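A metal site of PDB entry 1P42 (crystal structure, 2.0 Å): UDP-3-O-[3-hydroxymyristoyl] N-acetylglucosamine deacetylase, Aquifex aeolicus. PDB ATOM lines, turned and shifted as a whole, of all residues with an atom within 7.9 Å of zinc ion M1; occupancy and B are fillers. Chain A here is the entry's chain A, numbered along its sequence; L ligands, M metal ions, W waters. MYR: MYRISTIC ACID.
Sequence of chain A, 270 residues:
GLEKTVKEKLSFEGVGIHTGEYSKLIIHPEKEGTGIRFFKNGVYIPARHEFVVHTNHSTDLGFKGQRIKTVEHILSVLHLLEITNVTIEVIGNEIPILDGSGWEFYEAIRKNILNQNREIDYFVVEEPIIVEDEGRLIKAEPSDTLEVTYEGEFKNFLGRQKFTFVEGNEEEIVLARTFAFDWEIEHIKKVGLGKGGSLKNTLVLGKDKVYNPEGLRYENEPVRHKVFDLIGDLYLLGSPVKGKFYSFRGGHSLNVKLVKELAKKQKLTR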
ATOM      1  N   HIS A  57      19.462  18.640   6.980  1.00  0.00           N
ATOM      2  CA  HIS A  57      20.014  17.299   7.138  1.00  0.00           C
ATOM      3  C   HIS A  57      20.694  17.092   8.473  1.00  0.00           C
ATOM      4  O   HIS A  57      21.461  16.146   8.666  1.00  0.00           O
ATOM      5  CB  HIS A  57      20.967  17.025   5.971  1.00  0.00           C
ATOM      6  CG  HIS A  57      20.282  17.060   4.639  1.00  0.00           C
ATOM      7  ND1 HIS A  57      19.388  16.096   4.238  1.00  0.00           N
ATOM      8  CD2 HIS A  57      20.300  17.995   3.659  1.00  0.00           C
ATOM      9  CE1 HIS A  57      18.866  16.426   3.068  1.00  0.00           C
ATOM     10  NE2 HIS A  57      19.405  17.579   2.697  1.00  0.00           N
ATOM     11  N   SER A  58      20.394  17.984   9.404  1.00  0.00           N
ATOM     12  CA  SER A  58      20.928  17.950  10.761  1.00  0.00           C
ATOM     13  C   SER A  58      20.451  19.223  11.446  1.00  0.00           C
ATOM     14  O   SER A  58      19.912  20.110  10.791  1.00  0.00           O
ATOM     15  CB  SER A  58      22.464  17.889  10.741  1.00  0.00           C
ATOM     16  OG  SER A  58      23.043  19.018  10.109  1.00  0.00           O
ATOM     17  N   THR A  59      20.626  19.302  12.757  1.00  0.00           N
ATOM     18  CA  THR A  59      20.242  20.503  13.490  1.00  0.00           C
ATOM     19  C   THR A  59      21.548  21.223  13.791  1.00  0.00           C
ATOM     20  O   THR A  59      22.393  20.692  14.514  1.00  0.00           O
ATOM     21  CB  THR A  59      19.500  20.145  14.801  1.00  0.00           C
ATOM     22  OG1 THR A  59      18.314  19.404  14.478  1.00  0.00           O
ATOM     23  CG2 THR A  59      19.092  21.422  15.545  1.00  0.00           C
ATOM     24  N   THR A  70      25.163  19.379  13.527  1.00  0.00           N
ATOM     25  CA  THR A  70      24.700  18.109  14.075  1.00  0.00           C
ATOM     26  C   THR A  70      24.709  17.965  15.591  1.00  0.00           C
ATOM     27  O   THR A  70      25.376  17.073  16.134  1.00  0.00           O
ATOM     28  CB  THR A  70      25.541  16.965  13.453  1.00  0.00           C
ATOM     29  OG1 THR A  70      25.763  17.270  12.073  1.00  0.00           O
ATOM     30  CG2 THR A  70      24.817  15.610  13.561  1.00  0.00           C
ATOM     31  N   GLU A  72      21.914  17.371  17.368  1.00  0.00           N
ATOM     32  CA  GLU A  72      20.765  16.583  17.811  1.00  0.00           C
ATOM     33  C   GLU A  72      20.996  15.369  18.719  1.00  0.00           C
ATOM     34  O   GLU A  72      20.194  15.125  19.624  1.00  0.00           O
ATOM     35  CB  GLU A  72      19.896  16.157  16.613  1.00  0.00           C
ATOM     36  CG  GLU A  72      20.630  15.305  15.575  1.00  0.00           C
ATOM     37  CD  GLU A  72      21.120  16.105  14.383  1.00  0.00           C
ATOM     38  OE1 GLU A  72      21.623  17.226  14.586  1.00  0.00           O
ATOM     39  OE2 GLU A  72      21.039  15.597  13.238  1.00  0.00           O
ATOM     40  N   HIS A  73      22.067  14.616  18.483  1.00  0.00           N
ATOM     41  CA  HIS A  73      22.310  13.410  19.284  1.00  0.00           C
ATOM     42  C   HIS A  73      22.890  13.673  20.667  1.00  0.00           C
ATOM     43  O   HIS A  73      22.443  13.089  21.642  1.00  0.00           O
ATOM     44  CB  HIS A  73      23.192  12.432  18.495  1.00  0.00           C
ATOM     45  CG  HIS A  73      22.599  12.027  17.184  1.00  0.00           C
ATOM     46  ND1 HIS A  73      23.310  11.347  16.222  1.00  0.00           N
ATOM     47  CD2 HIS A  73      21.363  12.221  16.666  1.00  0.00           C
ATOM     48  CE1 HIS A  73      22.549  11.137  15.166  1.00  0.00           C
ATOM     49  NE2 HIS A  73      21.358  11.659  15.407  1.00  0.00           N
ATOM     50  N   SER A  76      20.129  15.114  22.690  1.00  0.00           N
ATOM     51  CA  SER A  76      19.092  14.168  23.083  1.00  0.00           C
ATOM     52  C   SER A  76      19.538  13.360  24.306  1.00  0.00           C
ATOM     53  O   SER A  76      18.755  13.121  25.220  1.00  0.00           O
ATOM     54  CB  SER A  76      18.766  13.210  21.936  1.00  0.00           C
ATOM     55  OG  SER A  76      17.699  12.343  22.304  1.00  0.00           O
ATOM     56  N   ILE A  97      29.989  12.014  14.879  1.00  0.00           N
ATOM     57  CA  ILE A  97      28.828  11.164  14.697  1.00  0.00           C
ATOM     58  C   ILE A  97      28.978   9.807  15.388  1.00  0.00           C
ATOM     59  O   ILE A  97      27.982   9.166  15.742  1.00  0.00           O
ATOM     60  CB  ILE A  97      28.554  10.925  13.174  1.00  0.00           C
ATOM     61  CG1 ILE A  97      27.236  10.175  12.983  1.00  0.00           C
ATOM     62  CG2 ILE A  97      29.697  10.147  12.543  1.00  0.00           C
ATOM     63  CD1 ILE A  97      26.010  10.957  13.406  1.00  0.00           C
ATOM     64  N   GLY A 100      26.586   6.718  14.933  1.00  0.00           N
ATOM     65  CA  GLY A 100      25.301   7.160  14.423  1.00  0.00           C
ATOM     66  C   GLY A 100      24.179   7.198  15.450  1.00  0.00           C
ATOM     67  O   GLY A 100      23.077   7.648  15.153  1.00  0.00           O
ATOM     68  N   SER A 101      24.448   6.716  16.663  1.00  0.00           N
ATOM     69  CA  SER A 101      23.447   6.713  17.737  1.00  0.00           C
ATOM     70  C   SER A 101      23.961   7.535  18.924  1.00  0.00           C
ATOM     71  O   SER A 101      24.976   8.230  18.815  1.00  0.00           O
ATOM     72  CB  SER A 101      23.138   5.282  18.199  1.00  0.00           C
ATOM     73  OG  SER A 101      24.199   4.739  18.975  1.00  0.00           O
ATOM     74  N   ALA A 176      19.591   3.370  18.680  1.00  0.00           N
ATOM     75  CA  ALA A 176      19.073   3.495  17.322  1.00  0.00           C
ATOM     76  C   ALA A 176      19.940   4.457  16.513  1.00  0.00           C
ATOM     77  O   ALA A 176      20.120   5.618  16.887  1.00  0.00           O
ATOM     78  CB  ALA A 176      17.620   3.975  17.344  1.00  0.00           C
ATOM     79  N   ARG A 177      20.459   3.972  15.384  1.00  0.00           N
ATOM     80  CA  ARG A 177      21.334   4.753  14.526  1.00  0.00           C
ATOM     81  C   ARG A 177      20.634   5.601  13.482  1.00  0.00           C
ATOM     82  O   ARG A 177      19.517   5.301  13.049  1.00  0.00           O
ATOM     83  CB  ARG A 177      22.307   3.827  13.797  1.00  0.00           C
ATOM     84  CG  ARG A 177      23.188   3.004  14.706  1.00  0.00           C
ATOM     85  CD  ARG A 177      23.767   1.854  13.913  1.00  0.00           C
ATOM     86  NE  ARG A 177      22.722   0.954  13.461  1.00  0.00           N
ATOM     87  CZ  ARG A 177      22.898  -0.029  12.585  1.00  0.00           C
ATOM     88  NH1 ARG A 177      24.101  -0.242  12.062  1.00  0.00           N
ATOM     89  NH2 ARG A 177      21.882  -0.810  12.252  1.00  0.00           N
ATOM     90  N   THR A 178      21.314   6.668  13.065  1.00  0.00           N
ATOM     91  CA  THR A 178      20.805   7.564  12.046  1.00  0.00           C
ATOM     92  C   THR A 178      20.741   6.721  10.772  1.00  0.00           C
ATOM     93  O   THR A 178      21.507   5.762  10.606  1.00  0.00           O
ATOM     94  CB  THR A 178      21.753   8.770  11.856  1.00  0.00           C
ATOM     95  OG1 THR A 178      21.252   9.618  10.823  1.00  0.00           O
ATOM     96  CG2 THR A 178      23.145   8.302  11.470  1.00  0.00           C
ATOM     97  N   PHE A 179      19.829   7.055   9.867  1.00  0.00           N
ATOM     98  CA  PHE A 179      19.670   6.291   8.638  1.00  0.00           C
ATOM     99  C   PHE A 179      19.394   7.191   7.453  1.00  0.00           C
ATOM    100  O   PHE A 179      18.994   8.354   7.615  1.00  0.00           O
ATOM    101  CB  PHE A 179      18.519   5.287   8.805  1.00  0.00           C
ATOM    102  CG  PHE A 179      17.166   5.939   8.970  1.00  0.00           C
ATOM    103  CD1 PHE A 179      16.340   6.159   7.871  1.00  0.00           C
ATOM    104  CD2 PHE A 179      16.739   6.360  10.227  1.00  0.00           C
ATOM    105  CE1 PHE A 179      15.113   6.792   8.006  1.00  0.00           C
ATOM    106  CE2 PHE A 179      15.507   7.009  10.380  1.00  0.00           C
ATOM    107  CZ  PHE A 179      14.690   7.224   9.272  1.00  0.00           C
ATOM    108  N   HIS A 225      15.003   5.933  16.065  1.00  0.00           N
ATOM    109  CA  HIS A 225      15.987   6.998  15.903  1.00  0.00           C
ATOM    110  C   HIS A 225      15.298   8.347  15.744  1.00  0.00           C
ATOM    111  O   HIS A 225      15.785   9.356  16.244  1.00  0.00           O
ATOM    112  CB  HIS A 225      16.892   6.768  14.692  1.00  0.00           C
ATOM    113  CG  HIS A 225      18.002   7.766  14.616  1.00  0.00           C
ATOM    114  ND1 HIS A 225      19.131   7.687  15.415  1.00  0.00           N
ATOM    115  CD2 HIS A 225      18.116   8.923  13.922  1.00  0.00           C
ATOM    116  CE1 HIS A 225      19.878   8.754  15.220  1.00  0.00           C
ATOM    117  NE2 HIS A 225      19.290   9.522  14.317  1.00  0.00           N
ATOM    118  N   LYS A 226      14.159   8.365  15.044  1.00  0.00           N
ATOM    119  CA  LYS A 226      13.430   9.611  14.854  1.00  0.00           C
ATOM    120  C   LYS A 226      12.902  10.124  16.202  1.00  0.00           C
ATOM    121  O   LYS A 226      12.840  11.335  16.421  1.00  0.00           O
ATOM    122  CB  LYS A 226      12.275   9.410  13.877  1.00  0.00           C
ATOM    123  CG  LYS A 226      12.711   9.286  12.422  1.00  0.00           C
ATOM    124  CD  LYS A 226      13.363  10.559  11.907  1.00  0.00           C
ATOM    125  CE  LYS A 226      13.765  10.426  10.442  1.00  0.00           C
ATOM    126  NZ  LYS A 226      14.387  11.663   9.892  1.00  0.00           N
ATOM    127  N   PHE A 228      14.422   9.595  19.000  1.00  0.00           N
ATOM    128  CA  PHE A 228      15.661  10.057  19.611  1.00  0.00           C
ATOM    129  C   PHE A 228      15.987  11.467  19.109  1.00  0.00           C
ATOM    130  O   PHE A 228      16.372  12.335  19.908  1.00  0.00           O
ATOM    131  CB  PHE A 228      16.783   9.072  19.255  1.00  0.00           C
ATOM    132  CG  PHE A 228      18.130   9.439  19.810  1.00  0.00           C
ATOM    133  CD1 PHE A 228      18.365   9.410  21.191  1.00  0.00           C
ATOM    134  CD2 PHE A 228      19.179   9.787  18.955  1.00  0.00           C
ATOM    135  CE1 PHE A 228      19.621   9.722  21.701  1.00  0.00           C
ATOM    136  CE2 PHE A 228      20.448  10.104  19.465  1.00  0.00           C
ATOM    137  CZ  PHE A 228      20.669  10.070  20.845  1.00  0.00           C
ATOM    138  N   ASP A 229      15.822  11.708  17.812  1.00  0.00           N
ATOM    139  CA  ASP A 229      16.083  13.034  17.232  1.00  0.00           C
ATOM    140  C   ASP A 229      15.157  14.104  17.806  1.00  0.00           C
ATOM    141  O   ASP A 229      15.606  15.197  18.153  1.00  0.00           O
ATOM    142  CB  ASP A 229      15.869  13.026  15.717  1.00  0.00           C
ATOM    143  CG  ASP A 229      17.019  12.417  14.961  1.00  0.00           C
ATOM    144  OD1 ASP A 229      18.129  12.335  15.522  1.00  0.00           O
ATOM    145  OD2 ASP A 229      16.809  12.041  13.791  1.00  0.00           O
ATOM    146  N   LEU A 230      13.863  13.813  17.864  1.00  0.00           N
ATOM    147  CA  LEU A 230      12.894  14.773  18.369  1.00  0.00           C
ATOM    148  C   LEU A 230      13.205  15.174  19.810  1.00  0.00           C
ATOM    149  O   LEU A 230      13.106  16.352  20.174  1.00  0.00           O
ATOM    150  CB  LEU A 230      11.476  14.178  18.271  1.00  0.00           C
ATOM    151  CG  LEU A 230      10.303  15.000  18.830  1.00  0.00           C
ATOM    152  CD1 LEU A 230      10.346  16.437  18.320  1.00  0.00           C
ATOM    153  CD2 LEU A 230       9.013  14.321  18.429  1.00  0.00           C
ATOM    154  N   ASP A 233      15.950  17.647  19.663  1.00  0.00           N
ATOM    155  CA  ASP A 233      15.494  18.956  19.210  1.00  0.00           C
ATOM    156  C   ASP A 233      14.630  19.659  20.250  1.00  0.00           C
ATOM    157  O   ASP A 233      14.653  20.879  20.379  1.00  0.00           O
ATOM    158  CB  ASP A 233      14.738  18.840  17.882  1.00  0.00           C
ATOM    159  CG  ASP A 233      15.666  18.506  16.705  1.00  0.00           C
ATOM    160  OD1 ASP A 233      16.849  18.895  16.745  1.00  0.00           O
ATOM    161  OD2 ASP A 233      15.201  17.860  15.731  1.00  0.00           O
ATOM    162  N   HIS A 252      13.833  17.256  11.577  1.00  0.00           N
ATOM    163  CA  HIS A 252      14.424  18.383  12.304  1.00  0.00           C
ATOM    164  C   HIS A 252      13.737  19.711  11.999  1.00  0.00           C
ATOM    165  O   HIS A 252      13.521  20.508  12.895  1.00  0.00           O
ATOM    166  CB  HIS A 252      15.926  18.491  11.994  1.00  0.00           C
ATOM    167  CG  HIS A 252      16.712  17.309  12.459  1.00  0.00           C
ATOM    168  ND1 HIS A 252      16.712  16.885  13.768  1.00  0.00           N
ATOM    169  CD2 HIS A 252      17.523  16.462  11.782  1.00  0.00           C
ATOM    170  CE1 HIS A 252      17.480  15.812  13.885  1.00  0.00           C
ATOM    171  NE2 HIS A 252      17.984  15.534  12.687  1.00  0.00           N
HETATM  172  C1  MYR L   1      19.138  13.924   9.411  1.00  0.00           C
HETATM  173  O1  MYR L   1      19.940  14.399  10.272  1.00  0.00           O
HETATM  174  O2  MYR L   1      17.877  13.967   9.513  1.00  0.00           O
HETATM  175  C2  MYR L   1      19.728  13.272   8.136  1.00  0.00           C
HETATM  176  C3  MYR L   1      20.528  12.032   8.450  1.00  0.00           C
HETATM  177  C4  MYR L   1      21.211  11.500   7.210  1.00  0.00           C
HETATM  178  C5  MYR L   1      22.689  11.831   7.212  1.00  0.00           C
HETATM  179  C6  MYR L   1      23.293  11.677   5.827  1.00  0.00           C
HETATM  180  C7  MYR L   1      24.285  10.539   5.795  1.00  0.00           C
HETATM  181  C8  MYR L   1      25.383  10.789   4.776  1.00  0.00           C
HETATM  182  C9  MYR L   1      25.311   9.833   3.606  1.00  0.00           C
HETATM  183  C10 MYR L   1      25.835   8.462   3.980  1.00  0.00           C
HETATM  184  C11 MYR L   1      26.633   7.822   2.869  1.00  0.00           C
HETATM  185  C12 MYR L   1      26.684   6.328   3.036  1.00  0.00           C
HETATM  186  C13 MYR L   1      27.863   5.711   2.322  1.00  0.00           C
HETATM  187  C14 MYR L   1      27.465   5.118   0.986  1.00  0.00           C
HETATM  188 ZN    ZN M   1      19.578  11.675  14.321  1.00  0.00          ZN
HETATM  189 ZN    ZN M   2      19.660  14.481  12.361  1.00  0.00          ZN
HETATM  190  O   HOH W   1      19.846  12.402  12.692  1.00  0.00           O
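A ring nitrogen (ND1) of His 225 sits close to the backbone NH (N) of Thr 178 (3.4 Å).
A ring nitrogen (ND1) of His 225 lies close to the backbone carbonyl oxygen of Arg 177, at 3.4 Å.
ND1 of His 225 sits at hydrogen-bond distance from O of Ala 176.
OE1 of Glu 72 is in hydrogen-bond range of N of Thr 59 (2.9 Å).
Residues that only touch zinc ion M1: Glu 72.
Within 4 Å of zinc ion M1: Glu 72, His 73, His 225 and Asp 229.
The nearest printed residue that does not touch zinc ion M1 is Thr 178 (4.4 Å).
Water W1 binds zinc ion M1, at 1.8 Å.
Zinc ion M1 is bound by OD1 of Asp 229, 2.0 Å away.
Zinc ion M1 is bound by NE2 of His 73 (2.1 Å).
A ring nitrogen (NE2) of His 225 binds zinc ion M1, at 2.2 Å.
Zinc ion M1 has four donor atoms within binding distance.
Slightly farther from zinc ion M1 lies OD2 of Asp 229 (2.8 Å).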
